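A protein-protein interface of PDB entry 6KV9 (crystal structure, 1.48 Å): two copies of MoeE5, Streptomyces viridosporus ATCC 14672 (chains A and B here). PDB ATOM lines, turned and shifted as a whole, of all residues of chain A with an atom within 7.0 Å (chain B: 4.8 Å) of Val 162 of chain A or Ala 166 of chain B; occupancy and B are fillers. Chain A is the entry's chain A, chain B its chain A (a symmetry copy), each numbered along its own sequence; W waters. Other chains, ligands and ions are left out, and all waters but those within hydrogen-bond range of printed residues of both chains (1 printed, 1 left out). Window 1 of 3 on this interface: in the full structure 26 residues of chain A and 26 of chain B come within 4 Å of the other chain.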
ATOM      1  N   PHE A 106      -4.016   2.155 -25.661  1.00  0.00           N
ATOM      2  CA  PHE A 106      -3.251   0.957 -25.342  1.00  0.00           C
ATOM      3  C   PHE A 106      -3.799  -0.341 -25.935  1.00  0.00           C
ATOM      4  O   PHE A 106      -2.988  -1.167 -26.407  1.00  0.00           O
ATOM      5  CB  PHE A 106      -3.017   0.871 -23.849  1.00  0.00           C
ATOM      6  CG  PHE A 106      -1.925  -0.113 -23.483  1.00  0.00           C
ATOM      7  CD1 PHE A 106      -0.609   0.041 -23.980  1.00  0.00           C
ATOM      8  CD2 PHE A 106      -2.220  -1.188 -22.639  1.00  0.00           C
ATOM      9  CE1 PHE A 106       0.397  -0.884 -23.611  1.00  0.00           C
ATOM     10  CE2 PHE A 106      -1.227  -2.111 -22.304  1.00  0.00           C
ATOM     11  CZ  PHE A 106       0.082  -1.974 -22.775  1.00  0.00           C
ATOM     12  N   LEU A 110      -1.291  -2.774 -28.074  1.00  0.00           N
ATOM     13  CA  LEU A 110      -1.094  -4.198 -27.789  1.00  0.00           C
ATOM     14  C   LEU A 110      -1.426  -5.058 -28.996  1.00  0.00           C
ATOM     15  O   LEU A 110      -0.726  -6.027 -29.323  1.00  0.00           O
ATOM     16  CB  LEU A 110      -1.996  -4.641 -26.641  1.00  0.00           C
ATOM     17  CG  LEU A 110      -1.529  -4.279 -25.249  1.00  0.00           C
ATOM     18  CD1 LEU A 110      -2.543  -4.805 -24.171  1.00  0.00           C
ATOM     19  CD2 LEU A 110      -0.103  -4.916 -24.955  1.00  0.00           C
ATOM     20  N   VAL A 114       2.148  -6.240 -30.182  1.00  0.00           N
ATOM     21  CA  VAL A 114       2.445  -7.457 -29.442  1.00  0.00           C
ATOM     22  C   VAL A 114       1.695  -8.659 -29.998  1.00  0.00           C
ATOM     23  O   VAL A 114       2.307  -9.663 -30.344  1.00  0.00           O
ATOM     24  CB  VAL A 114       2.194  -7.271 -27.932  1.00  0.00           C
ATOM     25  CG1 VAL A 114       2.750  -8.461 -27.140  1.00  0.00           C
ATOM     26  CG2 VAL A 114       2.876  -5.980 -27.423  1.00  0.00           C
ATOM     27  N   SER A 139      13.251   3.305 -27.207  1.00  0.00           N
ATOM     28  CA  SER A 139      12.354   3.536 -26.097  1.00  0.00           C
ATOM     29  C   SER A 139      12.297   2.364 -25.120  1.00  0.00           C
ATOM     30  O   SER A 139      11.848   2.556 -23.976  1.00  0.00           O
ATOM     31  CB  SER A 139      10.930   3.845 -26.571  1.00  0.00           C
ATOM     32  OG  SER A 139      10.384   2.754 -27.175  1.00  0.00           O
ATOM     33  N   VAL A 140      12.871   1.205 -25.475  1.00  0.00           N
ATOM     34  CA  VAL A 140      12.969   0.159 -24.439  1.00  0.00           C
ATOM     35  C   VAL A 140      13.921   0.530 -23.315  1.00  0.00           C
ATOM     36  O   VAL A 140      13.766   0.047 -22.175  1.00  0.00           O
ATOM     37  CB  VAL A 140      13.365  -1.219 -25.039  1.00  0.00           C
ATOM     38  CG1 VAL A 140      12.440  -1.633 -26.169  1.00  0.00           C
ATOM     39  CG2 VAL A 140      14.863  -1.279 -25.463  1.00  0.00           C
ATOM     40  N   ARG A 155      14.070  -0.298 -19.191  1.00  0.00           N
ATOM     41  CA  ARG A 155      13.248   0.375 -18.184  1.00  0.00           C
ATOM     42  C   ARG A 155      12.332   1.365 -18.901  1.00  0.00           C
ATOM     43  O   ARG A 155      12.396   2.580 -18.664  1.00  0.00           O
ATOM     44  CB  ARG A 155      14.138   1.096 -17.148  1.00  0.00           C
ATOM     45  CG  ARG A 155      15.030   0.138 -16.314  1.00  0.00           C
ATOM     46  CD  ARG A 155      16.066   0.920 -15.496  1.00  0.00           C
ATOM     47  NE  ARG A 155      16.735  -0.001 -14.576  1.00  0.00           N
ATOM     48  CZ  ARG A 155      17.722   0.322 -13.742  1.00  0.00           C
ATOM     49  NH1 ARG A 155      18.185   1.573 -13.684  1.00  0.00           N
ATOM     50  NH2 ARG A 155      18.241  -0.618 -12.953  1.00  0.00           N
ATOM     51  N   PRO A 156      11.496   0.885 -19.832  1.00  0.00           N
ATOM     52  CA  PRO A 156      10.691   1.835 -20.639  1.00  0.00           C
ATOM     53  C   PRO A 156       9.807   2.727 -19.793  1.00  0.00           C
ATOM     54  O   PRO A 156       9.253   2.330 -18.765  1.00  0.00           O
ATOM     55  CB  PRO A 156       9.852   0.930 -21.557  1.00  0.00           C
ATOM     56  CG  PRO A 156       9.885  -0.428 -20.876  1.00  0.00           C
ATOM     57  CD  PRO A 156      11.217  -0.535 -20.161  1.00  0.00           C
ATOM     58  N   LEU A 157       9.676   3.975 -20.238  1.00  0.00           N
ATOM     59  CA  LEU A 157       8.872   4.960 -19.529  1.00  0.00           C
ATOM     60  C   LEU A 157       7.539   5.241 -20.225  1.00  0.00           C
ATOM     61  O   LEU A 157       6.754   6.052 -19.713  1.00  0.00           O
ATOM     62  CB  LEU A 157       9.675   6.272 -19.398  1.00  0.00           C
ATOM     63  CG  LEU A 157      10.886   6.125 -18.476  1.00  0.00           C
ATOM     64  CD1 LEU A 157      11.544   7.494 -18.322  1.00  0.00           C
ATOM     65  CD2 LEU A 157      10.476   5.574 -17.135  1.00  0.00           C
ATOM     66  N   SER A 158       7.254   4.621 -21.365  1.00  0.00           N
ATOM     67  CA  SER A 158       5.954   4.754 -22.026  1.00  0.00           C
ATOM     68  C   SER A 158       5.356   3.380 -22.296  1.00  0.00           C
ATOM     69  O   SER A 158       6.094   2.386 -22.476  1.00  0.00           O
ATOM     70  CB  SER A 158       6.069   5.486 -23.367  1.00  0.00           C
ATOM     71  OG  SER A 158       6.933   4.789 -24.266  1.00  0.00           O
ATOM     72  N   PRO A 159       4.030   3.280 -22.382  1.00  0.00           N
ATOM     73  CA  PRO A 159       3.431   1.992 -22.809  1.00  0.00           C
ATOM     74  C   PRO A 159       3.927   1.557 -24.183  1.00  0.00           C
ATOM     75  O   PRO A 159       4.113   0.355 -24.411  1.00  0.00           O
ATOM     76  CB  PRO A 159       1.911   2.275 -22.796  1.00  0.00           C
ATOM     77  CG  PRO A 159       1.767   3.410 -21.775  1.00  0.00           C
ATOM     78  CD  PRO A 159       2.997   4.280 -21.993  1.00  0.00           C
ATOM     79  N   TYR A 160       4.189   2.474 -25.111  1.00  0.00           N
ATOM     80  CA  TYR A 160       4.793   2.116 -26.387  1.00  0.00           C
ATOM     81  C   TYR A 160       6.106   1.375 -26.172  1.00  0.00           C
ATOM     82  O   TYR A 160       6.337   0.316 -26.766  1.00  0.00           O
ATOM     83  CB  TYR A 160       5.036   3.391 -27.246  1.00  0.00           C
ATOM     84  CG  TYR A 160       5.905   3.155 -28.433  1.00  0.00           C
ATOM     85  CD1 TYR A 160       5.467   2.403 -29.528  1.00  0.00           C
ATOM     86  CD2 TYR A 160       7.237   3.621 -28.454  1.00  0.00           C
ATOM     87  CE1 TYR A 160       6.257   2.188 -30.637  1.00  0.00           C
ATOM     88  CE2 TYR A 160       8.038   3.376 -29.578  1.00  0.00           C
ATOM     89  CZ  TYR A 160       7.563   2.673 -30.665  1.00  0.00           C
ATOM     90  OH  TYR A 160       8.327   2.486 -31.780  1.00  0.00           O
ATOM     91  N   GLY A 161       6.982   1.936 -25.334  1.00  0.00           N
ATOM     92  CA  GLY A 161       8.256   1.253 -25.080  1.00  0.00           C
ATOM     93  C   GLY A 161       8.052  -0.150 -24.525  1.00  0.00           C
ATOM     94  O   GLY A 161       8.806  -1.074 -24.869  1.00  0.00           O
ATOM     95  N   VAL A 162       7.051  -0.305 -23.650  1.00  0.00           N
ATOM     96  CA  VAL A 162       6.741  -1.661 -23.139  1.00  0.00           C
ATOM     97  C   VAL A 162       6.309  -2.571 -24.273  1.00  0.00           C
ATOM     98  O   VAL A 162       6.734  -3.728 -24.338  1.00  0.00           O
ATOM     99  CB  VAL A 162       5.647  -1.572 -22.043  1.00  0.00           C
ATOM    100  CG1 VAL A 162       5.172  -3.019 -21.640  1.00  0.00           C
ATOM    101  CG2 VAL A 162       6.135  -0.812 -20.790  1.00  0.00           C
ATOM    102  N   THR A 163       5.500  -2.075 -25.213  1.00  0.00           N
ATOM    103  CA  THR A 163       5.065  -2.980 -26.294  1.00  0.00           C
ATOM    104  C   THR A 163       6.208  -3.358 -27.218  1.00  0.00           C
ATOM    105  O   THR A 163       6.255  -4.494 -27.694  1.00  0.00           O
ATOM    106  CB  THR A 163       3.898  -2.385 -27.141  1.00  0.00           C
ATOM    107  OG1 THR A 163       4.335  -1.219 -27.881  1.00  0.00           O
ATOM    108  CG2 THR A 163       2.681  -2.028 -26.270  1.00  0.00           C
ATOM    109  N   LYS A 164       7.171  -2.443 -27.454  1.00  0.00           N
ATOM    110  CA  LYS A 164       8.298  -2.811 -28.305  1.00  0.00           C
ATOM    111  C   LYS A 164       9.223  -3.774 -27.585  1.00  0.00           C
ATOM    112  O   LYS A 164       9.703  -4.733 -28.211  1.00  0.00           O
ATOM    113  CB  LYS A 164       9.089  -1.567 -28.732  1.00  0.00           C
ATOM    114  CG  LYS A 164       8.222  -0.574 -29.562  1.00  0.00           C
ATOM    115  CD  LYS A 164       7.673  -1.206 -30.853  1.00  0.00           C
ATOM    116  CE  LYS A 164       8.788  -1.731 -31.755  1.00  0.00           C
ATOM    117  NZ  LYS A 164       8.257  -2.120 -33.139  1.00  0.00           N
ATOM    118  N   LEU A 165       9.429  -3.577 -26.272  1.00  0.00           N
ATOM    119  CA  LEU A 165      10.162  -4.574 -25.471  1.00  0.00           C
ATOM    120  C   LEU A 165       9.489  -5.934 -25.531  1.00  0.00           C
ATOM    121  O   LEU A 165      10.165  -6.969 -25.696  1.00  0.00           O
ATOM    122  CB  LEU A 165      10.261  -4.085 -24.028  1.00  0.00           C
ATOM    123  CG  LEU A 165      10.981  -5.067 -23.048  1.00  0.00           C
ATOM    124  CD1 LEU A 165      12.466  -5.301 -23.480  1.00  0.00           C
ATOM    125  CD2 LEU A 165      10.908  -4.489 -21.661  1.00  0.00           C
ATOM    126  N   ALA A 166       8.156  -5.971 -25.362  1.00  0.00           N
ATOM    127  CA  ALA A 166       7.456  -7.256 -25.430  1.00  0.00           C
ATOM    128  C   ALA A 166       7.587  -7.891 -26.804  1.00  0.00           C
ATOM    129  O   ALA A 166       7.781  -9.103 -26.906  1.00  0.00           O
ATOM    130  CB  ALA A 166       5.984  -6.983 -25.062  1.00  0.00           C
ATOM    131  N   ALA A 167       7.478  -7.102 -27.886  1.00  0.00           N
ATOM    132  CA  ALA A 167       7.645  -7.672 -29.221  1.00  0.00           C
ATOM    133  C   ALA A 167       9.037  -8.290 -29.417  1.00  0.00           C
ATOM    134  O   ALA A 167       9.163  -9.409 -29.926  1.00  0.00           O
ATOM    135  CB  ALA A 167       7.366  -6.584 -30.252  1.00  0.00           C
ATOM    136  N   GLU A 168      10.099  -7.578 -29.004  1.00  0.00           N
ATOM    137  CA  GLU A 168      11.430  -8.138 -29.208  1.00  0.00           C
ATOM    138  C   GLU A 168      11.666  -9.345 -28.306  1.00  0.00           C
ATOM    139  O   GLU A 168      12.226 -10.337 -28.764  1.00  0.00           O
ATOM    140  CB  GLU A 168      12.488  -7.030 -29.105  1.00  0.00           C
ATOM    141  CG  GLU A 168      12.579  -6.374 -27.844  1.00  0.00           C
ATOM    142  CD  GLU A 168      14.038  -5.932 -27.528  1.00  0.00           C
ATOM    143  OE1 GLU A 168      14.568  -4.965 -28.144  1.00  0.00           O
ATOM    144  OE2 GLU A 168      14.699  -6.543 -26.667  1.00  0.00           O
ATOM    145  N   VAL B 114      -1.640  -7.993 -19.295  1.00  0.00           N
ATOM    146  CA  VAL B 114      -1.053  -6.732 -19.721  1.00  0.00           C
ATOM    147  C   VAL B 114      -2.088  -5.620 -19.801  1.00  0.00           C
ATOM    148  O   VAL B 114      -1.923  -4.576 -19.178  1.00  0.00           O
ATOM    149  CB  VAL B 114      -0.277  -6.892 -21.044  1.00  0.00           C
ATOM    150  CG1 VAL B 114       0.545  -5.633 -21.345  1.00  0.00           C
ATOM    151  CG2 VAL B 114       0.684  -8.100 -20.968  1.00  0.00           C
ATOM    152  N   VAL B 162       6.787 -13.260 -21.082  1.00  0.00           N
ATOM    153  CA  VAL B 162       6.749 -11.921 -21.717  1.00  0.00           C
ATOM    154  C   VAL B 162       5.620 -11.089 -21.138  1.00  0.00           C
ATOM    155  O   VAL B 162       5.805  -9.902 -20.857  1.00  0.00           O
ATOM    156  CB  VAL B 162       6.605 -12.072 -23.254  1.00  0.00           C
ATOM    157  CG1 VAL B 162       6.364 -10.661 -23.911  1.00  0.00           C
ATOM    158  CG2 VAL B 162       7.839 -12.745 -23.894  1.00  0.00           C
ATOM    159  N   THR B 163       4.448 -11.684 -20.904  1.00  0.00           N
ATOM    160  CA  THR B 163       3.351 -10.856 -20.368  1.00  0.00           C
ATOM    161  C   THR B 163       3.616 -10.408 -18.943  1.00  0.00           C
ATOM    162  O   THR B 163       3.251  -9.288 -18.581  1.00  0.00           O
ATOM    163  CB  THR B 163       1.970 -11.579 -20.429  1.00  0.00           C
ATOM    164  OG1 THR B 163       1.943 -12.725 -19.542  1.00  0.00           O
ATOM    165  CG2 THR B 163       1.612 -12.015 -21.860  1.00  0.00           C
ATOM    166  N   LYS B 164       4.290 -11.241 -18.124  1.00  0.00           N
ATOM    167  CA  LYS B 164       4.590 -10.801 -16.765  1.00  0.00           C
ATOM    168  C   LYS B 164       5.672  -9.737 -16.770  1.00  0.00           C
ATOM    169  O   LYS B 164       5.562  -8.760 -16.012  1.00  0.00           O
ATOM    170  CB  LYS B 164       5.041 -11.982 -15.895  1.00  0.00           C
ATOM    171  CG  LYS B 164       3.938 -13.074 -15.768  1.00  0.00           C
ATOM    172  CD  LYS B 164       2.645 -12.535 -15.132  1.00  0.00           C
ATOM    173  CE  LYS B 164       2.889 -11.941 -13.747  1.00  0.00           C
ATOM    174  NZ  LYS B 164       1.572 -11.645 -13.020  1.00  0.00           N
ATOM    175  N   LEU B 165       6.676  -9.873 -17.653  1.00  0.00           N
ATOM    176  CA  LEU B 165       7.658  -8.790 -17.844  1.00  0.00           C
ATOM    177  C   LEU B 165       6.980  -7.498 -18.265  1.00  0.00           C
ATOM    178  O   LEU B 165       7.306  -6.413 -17.743  1.00  0.00           O
ATOM    179  CB  LEU B 165       8.687  -9.223 -18.884  1.00  0.00           C
ATOM    180  CG  LEU B 165       9.773  -8.150 -19.221  1.00  0.00           C
ATOM    181  CD1 LEU B 165      10.625  -7.799 -17.958  1.00  0.00           C
ATOM    182  CD2 LEU B 165      10.643  -8.689 -20.325  1.00  0.00           C
ATOM    183  N   ALA B 166       6.056  -7.575 -19.237  1.00  0.00           N
ATOM    184  CA  ALA B 166       5.359  -6.359 -19.666  1.00  0.00           C
ATOM    185  C   ALA B 166       4.537  -5.760 -18.538  1.00  0.00           C
ATOM    186  O   ALA B 166       4.515  -4.539 -18.375  1.00  0.00           O
ATOM    187  CB  ALA B 166       4.480  -6.750 -20.871  1.00  0.00           C
ATOM    188  N   ALA B 167       3.842  -6.589 -17.743  1.00  0.00           N
ATOM    189  CA  ALA B 167       3.078  -6.049 -16.620  1.00  0.00           C
ATOM    190  C   ALA B 167       3.973  -5.316 -15.610  1.00  0.00           C
ATOM    191  O   ALA B 167       3.649  -4.207 -15.171  1.00  0.00           O
ATOM    192  CB  ALA B 167       2.309  -7.189 -15.962  1.00  0.00           C
ATOM    193  N   GLU B 168       5.115  -5.917 -15.238  1.00  0.00           N
ATOM    194  CA  GLU B 168       5.963  -5.248 -14.258  1.00  0.00           C
ATOM    195  C   GLU B 168       6.606  -3.997 -14.847  1.00  0.00           C
ATOM    196  O   GLU B 168       6.661  -2.974 -14.170  1.00  0.00           O
ATOM    197  CB  GLU B 168       6.942  -6.254 -13.636  1.00  0.00           C
ATOM    198  CG  GLU B 168       7.866  -6.859 -14.536  1.00  0.00           C
ATOM    199  CD  GLU B 168       9.229  -7.159 -13.848  1.00  0.00           C
ATOM    200  OE1 GLU B 168       9.335  -8.095 -13.005  1.00  0.00           O
ATOM    201  OE2 GLU B 168      10.227  -6.465 -14.117  1.00  0.00           O
ATOM    202  N   ARG B 169       7.075  -4.063 -16.096  1.00  0.00           N
ATOM    203  CA  ARG B 169       7.645  -2.865 -16.712  1.00  0.00           C
ATOM    204  C   ARG B 169       6.616  -1.758 -16.832  1.00  0.00           C
ATOM    205  O   ARG B 169       6.941  -0.588 -16.624  1.00  0.00           O
ATOM    206  CB  ARG B 169       8.247  -3.185 -18.075  1.00  0.00           C
ATOM    207  CG  ARG B 169       9.448  -4.161 -18.046  1.00  0.00           C
ATOM    208  CD  ARG B 169      10.671  -3.559 -17.386  1.00  0.00           C
ATOM    209  NE  ARG B 169      10.862  -4.064 -16.034  1.00  0.00           N
ATOM    210  CZ  ARG B 169      11.859  -3.712 -15.226  1.00  0.00           C
ATOM    211  NH1 ARG B 169      11.919  -4.261 -14.006  1.00  0.00           N
ATOM    212  NH2 ARG B 169      12.754  -2.788 -15.603  1.00  0.00           N
ATOM    213  N   LEU B 170       5.371  -2.104 -17.167  1.00  0.00           N
ATOM    214  CA  LEU B 170       4.315  -1.089 -17.236  1.00  0.00           C
ATOM    215  C   LEU B 170       4.071  -0.461 -15.893  1.00  0.00           C
ATOM    216  O   LEU B 170       3.903   0.772 -15.773  1.00  0.00           O
ATOM    217  CB  LEU B 170       2.992  -1.738 -17.640  1.00  0.00           C
ATOM    218  CG  LEU B 170       2.583  -1.910 -19.066  1.00  0.00           C
ATOM    219  CD1 LEU B 170       1.351  -2.811 -19.116  1.00  0.00           C
ATOM    220  CD2 LEU B 170       2.286  -0.527 -19.673  1.00  0.00           C
HETATM  221  O   HOH W   1       9.634   0.084 -17.180  1.00  0.00           O
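Of the printed residues of chain B, Phe 106 of chain A touches Val 114 and Leu 170. Of the printed residues of chain B, Arg 155 of chain A touches Arg 169 (3.8 Å). Of the printed residues of chain B, Val 162 of chain A touches Ala 166 and Leu 170. Lys 164 of chain A touches none of the printed residues of chain B. Printed residues of chain B within 4 Å of Ala 166 of chain A: Val 162 (3.7 Å). Lys 164 of chain B touches none of the printed residues of chain A. Ala 166 of chain B touches just one residue of chain A: Val 162. Of the printed residues of chain A, Arg 169 of chain B touches Arg 155 and Leu 165. The nearest residue of chain A that does not touch Ala 166 of chain B is Ala 166 of chain A (4.5 Å).
O of Val 140 of chain A lies within hydrogen-bond range of N of Arg 155 of chain A, 3.0 Å away. The side-chain carboxylate (OE2) of Glu 168 of chain B is in salt-bridge range of the guanidinium group (NH1) of Arg 169 of chain B (2.8 Å).
Water W1 bridges the backbone carbonyl oxygen of Pro 156 of chain A (2.8 Å) and the backbone carbonyl oxygen of Arg 169 of chain B (2.8 Å).
Of the 10 printed residues of chain B, 5 touch a printed residue of chain A. Of the 19 printed residues of chain A, 6 touch a printed residue of chain B. Among the printed residues, 8 pairs touch across the chains. Among the printed residues, no Asp or Glu carboxylate lies within 4 Å of a Lys or Arg side-chain nitrogen of the other chain.
Phe 106 of chain A touches Val 114 of chain B (CZ to CG1, 3.96 Å). Phe 106 of chain A touches Leu 170 of chain B. Val 114 of chain B touches Leu 110 of chain A. Arg 155 of chain A touches Arg 169 of chain B. Val 162 of chain A touches Ala 166 of chain B (CG1 to O, 3.7 Å). Leu 170 of chain B touches Val 162 of chain A (CG to CG1, 3.8 Å). Arg 169 of chain B touches Leu 165 of chain A (CG to CD2, 3.9 Å). Ala 166 of chain A touches Val 162 of chain B.
Val 162 of chain A touches Ala 166 of chain B, and with the chains exchanged Ala 166 of chain A touches Val 162 of chain B. 8 positions are printed for both chains. Of the 8 pairs that touch across the chains among the printed residues, 2 have their exchanged pair printed and touching as well.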
